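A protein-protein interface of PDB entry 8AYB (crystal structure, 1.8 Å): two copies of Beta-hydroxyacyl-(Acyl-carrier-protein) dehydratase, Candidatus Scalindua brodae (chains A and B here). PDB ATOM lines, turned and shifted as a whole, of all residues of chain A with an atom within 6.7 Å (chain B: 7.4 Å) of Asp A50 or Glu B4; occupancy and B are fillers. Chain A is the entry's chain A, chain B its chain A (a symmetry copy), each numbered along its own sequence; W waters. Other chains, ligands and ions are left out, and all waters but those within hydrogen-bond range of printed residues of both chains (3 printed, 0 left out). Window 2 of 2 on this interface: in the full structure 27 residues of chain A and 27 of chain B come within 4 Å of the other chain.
Hydrophobic or aromatic side chains of chain B within 4 Å of the printed part of chain A: Phe B3. Along chain B the printed residues that touch a printed residue of chain A span positions 3 to 20. Among the printed residues, 8 pairs touch across the chains.
The side-chain amide oxygen (OD1) of Asn B2 lies close to the backbone NH (N) of Glu B4 (3.5 Å). N of Phe B3 sits close to O of Asp B20, 3.4 Å away. NH1 of Arg B7 is in salt-bridge range of OE1 of Glu B4, at 3.1 Å.
The backbone carbonyl oxygen (O) of Pro A49 lies within hydrogen-bond range of the guanidinium group (NH2) of Arg B7 (3.5 Å). OE1 of Glu B4 is in hydrogen-bond range of N of Ala A52. O of Asp A50 lies close to OE2 of Glu B4.
No position is printed for both chains. Of the 8 pairs that touch across the chains among the printed residues, none has its exchanged pair printed and touching as well.
Among the printed residues, pairs that only touch across the chains: Phe A51 with Glu B4 (3.3 Å), Pro A100 with Phe B3 (3.6 Å), Ala A52 with Arg B7 (3.6 Å), Pro A100 with Asp B20 (3.7 Å) and Phe A51 with Arg B7 (3.99 Å).
Asp A50 touches one residue of chain B. Glu B4 touches just these residues of chain A: Asp A50, Phe A51 and Ala A52. Printed residues of chain A within 4 Å of Arg B7: Pro A49, Phe A51 and Ala A52. Printed residues of chain B within 4 Å of Ala A52: Glu B4 (2.9 Å) and Arg B7 (3.6 Å). Printed residues of chain B within 4 Å of Phe A51: Glu B4 and Arg B7. Printed residues of chain A within 4 Å of Asp B20: Pro A100 (3.7 Å). Printed residues of chain B within 4 Å of Pro A49: Arg B7 (3.5 Å). The nearest residue of chain A that does not touch Glu B4 is Pro A49 (5.5 Å). The nearest printed residue of chain A that does not touch Phe B3 is Ala A52 (4.02 Å).
Water W3 lies within hydrogen-bond range of the backbone carbonyl oxygen (O) of Phe A48 and the guanidinium group (NH2) of Arg B7. Water W2 bridges O of Ala A52 and OE1 of Glu B4. Water W1 lies within hydrogen-bond range of the backbone carbonyl oxygen (O) of Pro A100 (2.8 Å) and the backbone NH (N) of Phe B3 (2.9 Å).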
ATOM      1  N   ALA A  45     -20.820  21.652  19.351  1.00  0.00           N
ATOM      2  CA  ALA A  45     -20.114  21.246  20.562  1.00  0.00           C
ATOM      3  C   ALA A  45     -19.713  19.771  20.527  1.00  0.00           C
ATOM      4  O   ALA A  45     -18.729  19.374  21.169  1.00  0.00           O
ATOM      5  CB  ALA A  45     -20.982  21.512  21.792  1.00  0.00           C
ATOM      6  N   HIS A  47     -19.276  17.943  17.536  1.00  0.00           N
ATOM      7  CA  HIS A  47     -18.782  17.515  16.222  1.00  0.00           C
ATOM      8  C   HIS A  47     -17.977  18.670  15.615  1.00  0.00           C
ATOM      9  O   HIS A  47     -18.479  19.457  14.813  1.00  0.00           O
ATOM     10  CB  HIS A  47     -19.935  17.110  15.303  1.00  0.00           C
ATOM     11  CG  HIS A  47     -19.506  16.474  14.014  1.00  0.00           C
ATOM     12  ND1 HIS A  47     -19.007  17.205  12.954  1.00  0.00           N
ATOM     13  CD2 HIS A  47     -19.527  15.184  13.605  1.00  0.00           C
ATOM     14  CE1 HIS A  47     -18.719  16.387  11.955  1.00  0.00           C
ATOM     15  NE2 HIS A  47     -19.029  15.157  12.323  1.00  0.00           N
ATOM     16  N   PHE A  48     -16.712  18.787  16.000  1.00  0.00           N
ATOM     17  CA  PHE A  48     -16.064  18.008  17.044  1.00  0.00           C
ATOM     18  C   PHE A  48     -15.595  18.971  18.121  1.00  0.00           C
ATOM     19  O   PHE A  48     -15.392  20.159  17.835  1.00  0.00           O
ATOM     20  CB  PHE A  48     -14.860  17.247  16.497  1.00  0.00           C
ATOM     21  CG  PHE A  48     -15.181  16.323  15.370  1.00  0.00           C
ATOM     22  CD1 PHE A  48     -15.610  15.025  15.620  1.00  0.00           C
ATOM     23  CD2 PHE A  48     -15.020  16.737  14.055  1.00  0.00           C
ATOM     24  CE1 PHE A  48     -15.889  14.163  14.589  1.00  0.00           C
ATOM     25  CE2 PHE A  48     -15.302  15.875  13.005  1.00  0.00           C
ATOM     26  CZ  PHE A  48     -15.736  14.579  13.271  1.00  0.00           C
ATOM     27  N   PRO A  49     -15.388  18.467  19.342  1.00  0.00           N
ATOM     28  CA  PRO A  49     -14.868  19.342  20.408  1.00  0.00           C
ATOM     29  C   PRO A  49     -13.654  20.161  19.986  1.00  0.00           C
ATOM     30  O   PRO A  49     -13.626  21.381  20.197  1.00  0.00           O
ATOM     31  CB  PRO A  49     -14.530  18.349  21.527  1.00  0.00           C
ATOM     32  CG  PRO A  49     -15.435  17.203  21.303  1.00  0.00           C
ATOM     33  CD  PRO A  49     -15.623  17.089  19.819  1.00  0.00           C
ATOM     34  N   ASP A  50     -12.658  19.517  19.372  1.00  0.00           N
ATOM     35  CA  ASP A  50     -11.428  20.191  18.972  1.00  0.00           C
ATOM     36  C   ASP A  50     -11.580  21.016  17.701  1.00  0.00           C
ATOM     37  O   ASP A  50     -10.707  21.841  17.406  1.00  0.00           O
ATOM     38  CB  ASP A  50     -10.302  19.173  18.742  1.00  0.00           C
ATOM     39  CG  ASP A  50      -9.783  18.558  20.031  1.00  0.00           C
ATOM     40  OD1 ASP A  50      -9.930  19.187  21.101  1.00  0.00           O
ATOM     41  OD2 ASP A  50      -9.213  17.446  19.969  1.00  0.00           O
ATOM     42  N   PHE A  51     -12.646  20.807  16.933  1.00  0.00           N
ATOM     43  CA  PHE A  51     -12.704  21.376  15.591  1.00  0.00           C
ATOM     44  C   PHE A  51     -14.151  21.322  15.125  1.00  0.00           C
ATOM     45  O   PHE A  51     -14.670  20.233  14.863  1.00  0.00           O
ATOM     46  CB  PHE A  51     -11.779  20.596  14.664  1.00  0.00           C
ATOM     47  CG  PHE A  51     -11.507  21.271  13.357  1.00  0.00           C
ATOM     48  CD1 PHE A  51     -10.831  22.469  13.302  1.00  0.00           C
ATOM     49  CD2 PHE A  51     -11.883  20.677  12.178  1.00  0.00           C
ATOM     50  CE1 PHE A  51     -10.568  23.088  12.082  1.00  0.00           C
ATOM     51  CE2 PHE A  51     -11.629  21.285  10.954  1.00  0.00           C
ATOM     52  CZ  PHE A  51     -10.969  22.493  10.910  1.00  0.00           C
ATOM     53  N   ALA A  52     -14.806  22.482  15.041  1.00  0.00           N
ATOM     54  CA  ALA A  52     -16.206  22.522  14.639  1.00  0.00           C
ATOM     55  C   ALA A  52     -16.314  22.367  13.122  1.00  0.00           C
ATOM     56  O   ALA A  52     -15.788  23.201  12.368  1.00  0.00           O
ATOM     57  CB  ALA A  52     -16.860  23.821  15.110  1.00  0.00           C
ATOM     58  N   ILE A  53     -16.976  21.300  12.676  1.00  0.00           N
ATOM     59  CA  ILE A  53     -17.236  21.037  11.253  1.00  0.00           C
ATOM     60  C   ILE A  53     -18.664  20.558  11.122  1.00  0.00           C
ATOM     61  O   ILE A  53     -19.097  19.702  11.896  1.00  0.00           O
ATOM     62  CB  ILE A  53     -16.344  19.940  10.643  1.00  0.00           C
ATOM     63  CG1 ILE A  53     -14.942  19.926  11.213  1.00  0.00           C
ATOM     64  CG2 ILE A  53     -16.283  20.083   9.108  1.00  0.00           C
ATOM     65  CD1 ILE A  53     -14.076  18.877  10.495  1.00  0.00           C
ATOM     66  N   PHE A  99     -18.230  25.025   7.502  1.00  0.00           N
ATOM     67  CA  PHE A  99     -17.750  25.557   8.770  1.00  0.00           C
ATOM     68  C   PHE A  99     -18.654  26.666   9.281  1.00  0.00           C
ATOM     69  O   PHE A  99     -19.359  27.309   8.499  1.00  0.00           O
ATOM     70  CB  PHE A  99     -16.322  26.112   8.623  1.00  0.00           C
ATOM     71  CG  PHE A  99     -15.326  25.079   8.215  1.00  0.00           C
ATOM     72  CD1 PHE A  99     -14.901  24.118   9.121  1.00  0.00           C
ATOM     73  CD2 PHE A  99     -14.843  25.041   6.918  1.00  0.00           C
ATOM     74  CE1 PHE A  99     -13.999  23.139   8.737  1.00  0.00           C
ATOM     75  CE2 PHE A  99     -13.942  24.071   6.533  1.00  0.00           C
ATOM     76  CZ  PHE A  99     -13.517  23.121   7.440  1.00  0.00           C
ATOM     77  N   PRO A 100     -18.632  26.936  10.588  1.00  0.00           N
ATOM     78  CA  PRO A 100     -19.253  28.168  11.089  1.00  0.00           C
ATOM     79  C   PRO A 100     -18.790  29.374  10.277  1.00  0.00           C
ATOM     80  O   PRO A 100     -17.609  29.514   9.954  1.00  0.00           O
ATOM     81  CB  PRO A 100     -18.776  28.228  12.540  1.00  0.00           C
ATOM     82  CG  PRO A 100     -18.657  26.746  12.922  1.00  0.00           C
ATOM     83  CD  PRO A 100     -18.052  26.133  11.685  1.00  0.00           C
ATOM     84  N   VAL B   1      -9.592  35.391   9.783  1.00  0.00           N
ATOM     85  CA  VAL B   1      -9.588  34.607  11.013  1.00  0.00           C
ATOM     86  C   VAL B   1     -10.845  33.749  11.049  1.00  0.00           C
ATOM     87  O   VAL B   1     -11.960  34.274  11.105  1.00  0.00           O
ATOM     88  CB  VAL B   1      -9.495  35.502  12.255  1.00  0.00           C
ATOM     89  CG1 VAL B   1      -9.455  34.668  13.513  1.00  0.00           C
ATOM     90  CG2 VAL B   1      -8.263  36.413  12.178  1.00  0.00           C
ATOM     91  N   ASN B   2     -10.661  32.433  10.998  1.00  0.00           N
ATOM     92  CA  ASN B   2     -11.780  31.508  10.954  1.00  0.00           C
ATOM     93  C   ASN B   2     -12.286  31.207  12.362  1.00  0.00           C
ATOM     94  O   ASN B   2     -11.722  31.649  13.372  1.00  0.00           O
ATOM     95  CB  ASN B   2     -11.396  30.216  10.228  1.00  0.00           C
ATOM     96  CG  ASN B   2     -10.257  29.458  10.911  1.00  0.00           C
ATOM     97  OD1 ASN B   2      -9.845  29.776  12.033  1.00  0.00           O
ATOM     98  ND2 ASN B   2      -9.740  28.445  10.223  1.00  0.00           N
ATOM     99  N   PHE B   3     -13.351  30.407  12.424  1.00  0.00           N
ATOM    100  CA  PHE B   3     -14.008  30.150  13.699  1.00  0.00           C
ATOM    101  C   PHE B   3     -13.060  29.504  14.697  1.00  0.00           C
ATOM    102  O   PHE B   3     -13.060  29.864  15.879  1.00  0.00           O
ATOM    103  CB  PHE B   3     -15.239  29.271  13.495  1.00  0.00           C
ATOM    104  CG  PHE B   3     -16.028  29.053  14.763  1.00  0.00           C
ATOM    105  CD1 PHE B   3     -16.607  30.128  15.417  1.00  0.00           C
ATOM    106  CD2 PHE B   3     -16.168  27.788  15.307  1.00  0.00           C
ATOM    107  CE1 PHE B   3     -17.325  29.944  16.596  1.00  0.00           C
ATOM    108  CE2 PHE B   3     -16.887  27.597  16.475  1.00  0.00           C
ATOM    109  CZ  PHE B   3     -17.469  28.681  17.119  1.00  0.00           C
ATOM    110  N   GLU B   4     -12.245  28.547  14.247  1.00  0.00           N
ATOM    111  CA  GLU B   4     -11.346  27.868  15.176  1.00  0.00           C
ATOM    112  C   GLU B   4     -10.408  28.849  15.862  1.00  0.00           C
ATOM    113  O   GLU B   4     -10.132  28.721  17.061  1.00  0.00           O
ATOM    114  CB  GLU B   4     -10.545  26.789  14.457  1.00  0.00           C
ATOM    115  CG  GLU B   4     -11.359  25.574  14.160  1.00  0.00           C
ATOM    116  CD  GLU B   4     -12.091  25.035  15.382  1.00  0.00           C
ATOM    117  OE1 GLU B   4     -13.343  24.997  15.341  1.00  0.00           O
ATOM    118  OE2 GLU B   4     -11.419  24.658  16.375  1.00  0.00           O
ATOM    119  N   GLU B   5      -9.903  29.834  15.118  1.00  0.00           N
ATOM    120  CA  GLU B   5      -9.048  30.842  15.733  1.00  0.00           C
ATOM    121  C   GLU B   5      -9.853  31.795  16.610  1.00  0.00           C
ATOM    122  O   GLU B   5      -9.388  32.204  17.679  1.00  0.00           O
ATOM    123  CB  GLU B   5      -8.302  31.619  14.655  1.00  0.00           C
ATOM    124  CG  GLU B   5      -7.253  30.833  13.901  1.00  0.00           C
ATOM    125  CD  GLU B   5      -6.661  31.641  12.759  1.00  0.00           C
ATOM    126  OE1 GLU B   5      -7.224  31.587  11.642  1.00  0.00           O
ATOM    127  OE2 GLU B   5      -5.651  32.348  12.988  1.00  0.00           O
ATOM    128  N   VAL B   6     -11.053  32.171  16.162  1.00  0.00           N
ATOM    129  CA  VAL B   6     -11.919  33.034  16.961  1.00  0.00           C
ATOM    130  C   VAL B   6     -12.191  32.397  18.319  1.00  0.00           C
ATOM    131  O   VAL B   6     -12.144  33.070  19.358  1.00  0.00           O
ATOM    132  CB  VAL B   6     -13.224  33.323  16.195  1.00  0.00           C
ATOM    133  CG1 VAL B   6     -14.242  34.007  17.093  1.00  0.00           C
ATOM    134  CG2 VAL B   6     -12.936  34.171  14.960  1.00  0.00           C
ATOM    135  N   ARG B   7     -12.448  31.083  18.329  1.00  0.00           N
ATOM    136  CA  ARG B   7     -12.746  30.370  19.571  1.00  0.00           C
ATOM    137  C   ARG B   7     -11.638  30.527  20.591  1.00  0.00           C
ATOM    138  O   ARG B   7     -11.902  30.572  21.796  1.00  0.00           O
ATOM    139  CB  ARG B   7     -12.937  28.881  19.313  1.00  0.00           C
ATOM    140  CG  ARG B   7     -14.131  28.493  18.543  1.00  0.00           C
ATOM    141  CD  ARG B   7     -14.026  27.012  18.263  1.00  0.00           C
ATOM    142  NE  ARG B   7     -14.764  26.212  19.227  1.00  0.00           N
ATOM    143  CZ  ARG B   7     -14.884  24.893  19.144  1.00  0.00           C
ATOM    144  NH1 ARG B   7     -14.292  24.235  18.155  1.00  0.00           N
ATOM    145  NH2 ARG B   7     -15.587  24.232  20.049  1.00  0.00           N
ATOM    146  N   GLU B   8     -10.387  30.543  20.133  1.00  0.00           N
ATOM    147  CA  GLU B   8      -9.269  30.645  21.059  1.00  0.00           C
ATOM    148  C   GLU B   8      -9.011  32.084  21.482  1.00  0.00           C
ATOM    149  O   GLU B   8      -8.549  32.320  22.604  1.00  0.00           O
ATOM    150  CB  GLU B   8      -8.016  30.029  20.436  1.00  0.00           C
ATOM    151  CG  GLU B   8      -7.010  29.525  21.459  1.00  0.00           C
ATOM    152  CD  GLU B   8      -7.669  28.769  22.606  1.00  0.00           C
ATOM    153  OE1 GLU B   8      -7.388  29.101  23.780  1.00  0.00           O
ATOM    154  OE2 GLU B   8      -8.472  27.848  22.334  1.00  0.00           O
ATOM    155  N   LEU B   9      -9.322  33.053  20.617  1.00  0.00           N
ATOM    156  CA  LEU B   9      -9.146  34.457  20.978  1.00  0.00           C
ATOM    157  C   LEU B   9     -10.181  34.903  22.002  1.00  0.00           C
ATOM    158  O   LEU B   9      -9.850  35.609  22.962  1.00  0.00           O
ATOM    159  CB  LEU B   9      -9.230  35.333  19.727  1.00  0.00           C
ATOM    160  CG  LEU B   9      -8.041  35.304  18.768  1.00  0.00           C
ATOM    161  CD1 LEU B   9      -8.388  36.005  17.464  1.00  0.00           C
ATOM    162  CD2 LEU B   9      -6.843  35.961  19.428  1.00  0.00           C
ATOM    163  N   ASP B  20     -18.490  34.463  14.307  1.00  0.00           N
ATOM    164  CA  ASP B  20     -18.099  33.326  13.483  1.00  0.00           C
ATOM    165  C   ASP B  20     -16.739  33.508  12.821  1.00  0.00           C
ATOM    166  O   ASP B  20     -15.942  32.567  12.787  1.00  0.00           O
ATOM    167  CB  ASP B  20     -19.165  33.053  12.427  1.00  0.00           C
ATOM    168  CG  ASP B  20     -20.385  32.387  13.024  1.00  0.00           C
ATOM    169  OD1 ASP B  20     -20.209  31.391  13.768  1.00  0.00           O
ATOM    170  OD2 ASP B  20     -21.511  32.868  12.777  1.00  0.00           O
HETATM  171  O   HOH W   1     -14.789  29.447  10.092  1.00  0.00           O
HETATM  172  O   HOH W   2     -14.666  25.622  12.790  1.00  0.00           O
HETATM  173  O   HOH W   3     -16.725  22.291  18.624  1.00  0.00           O
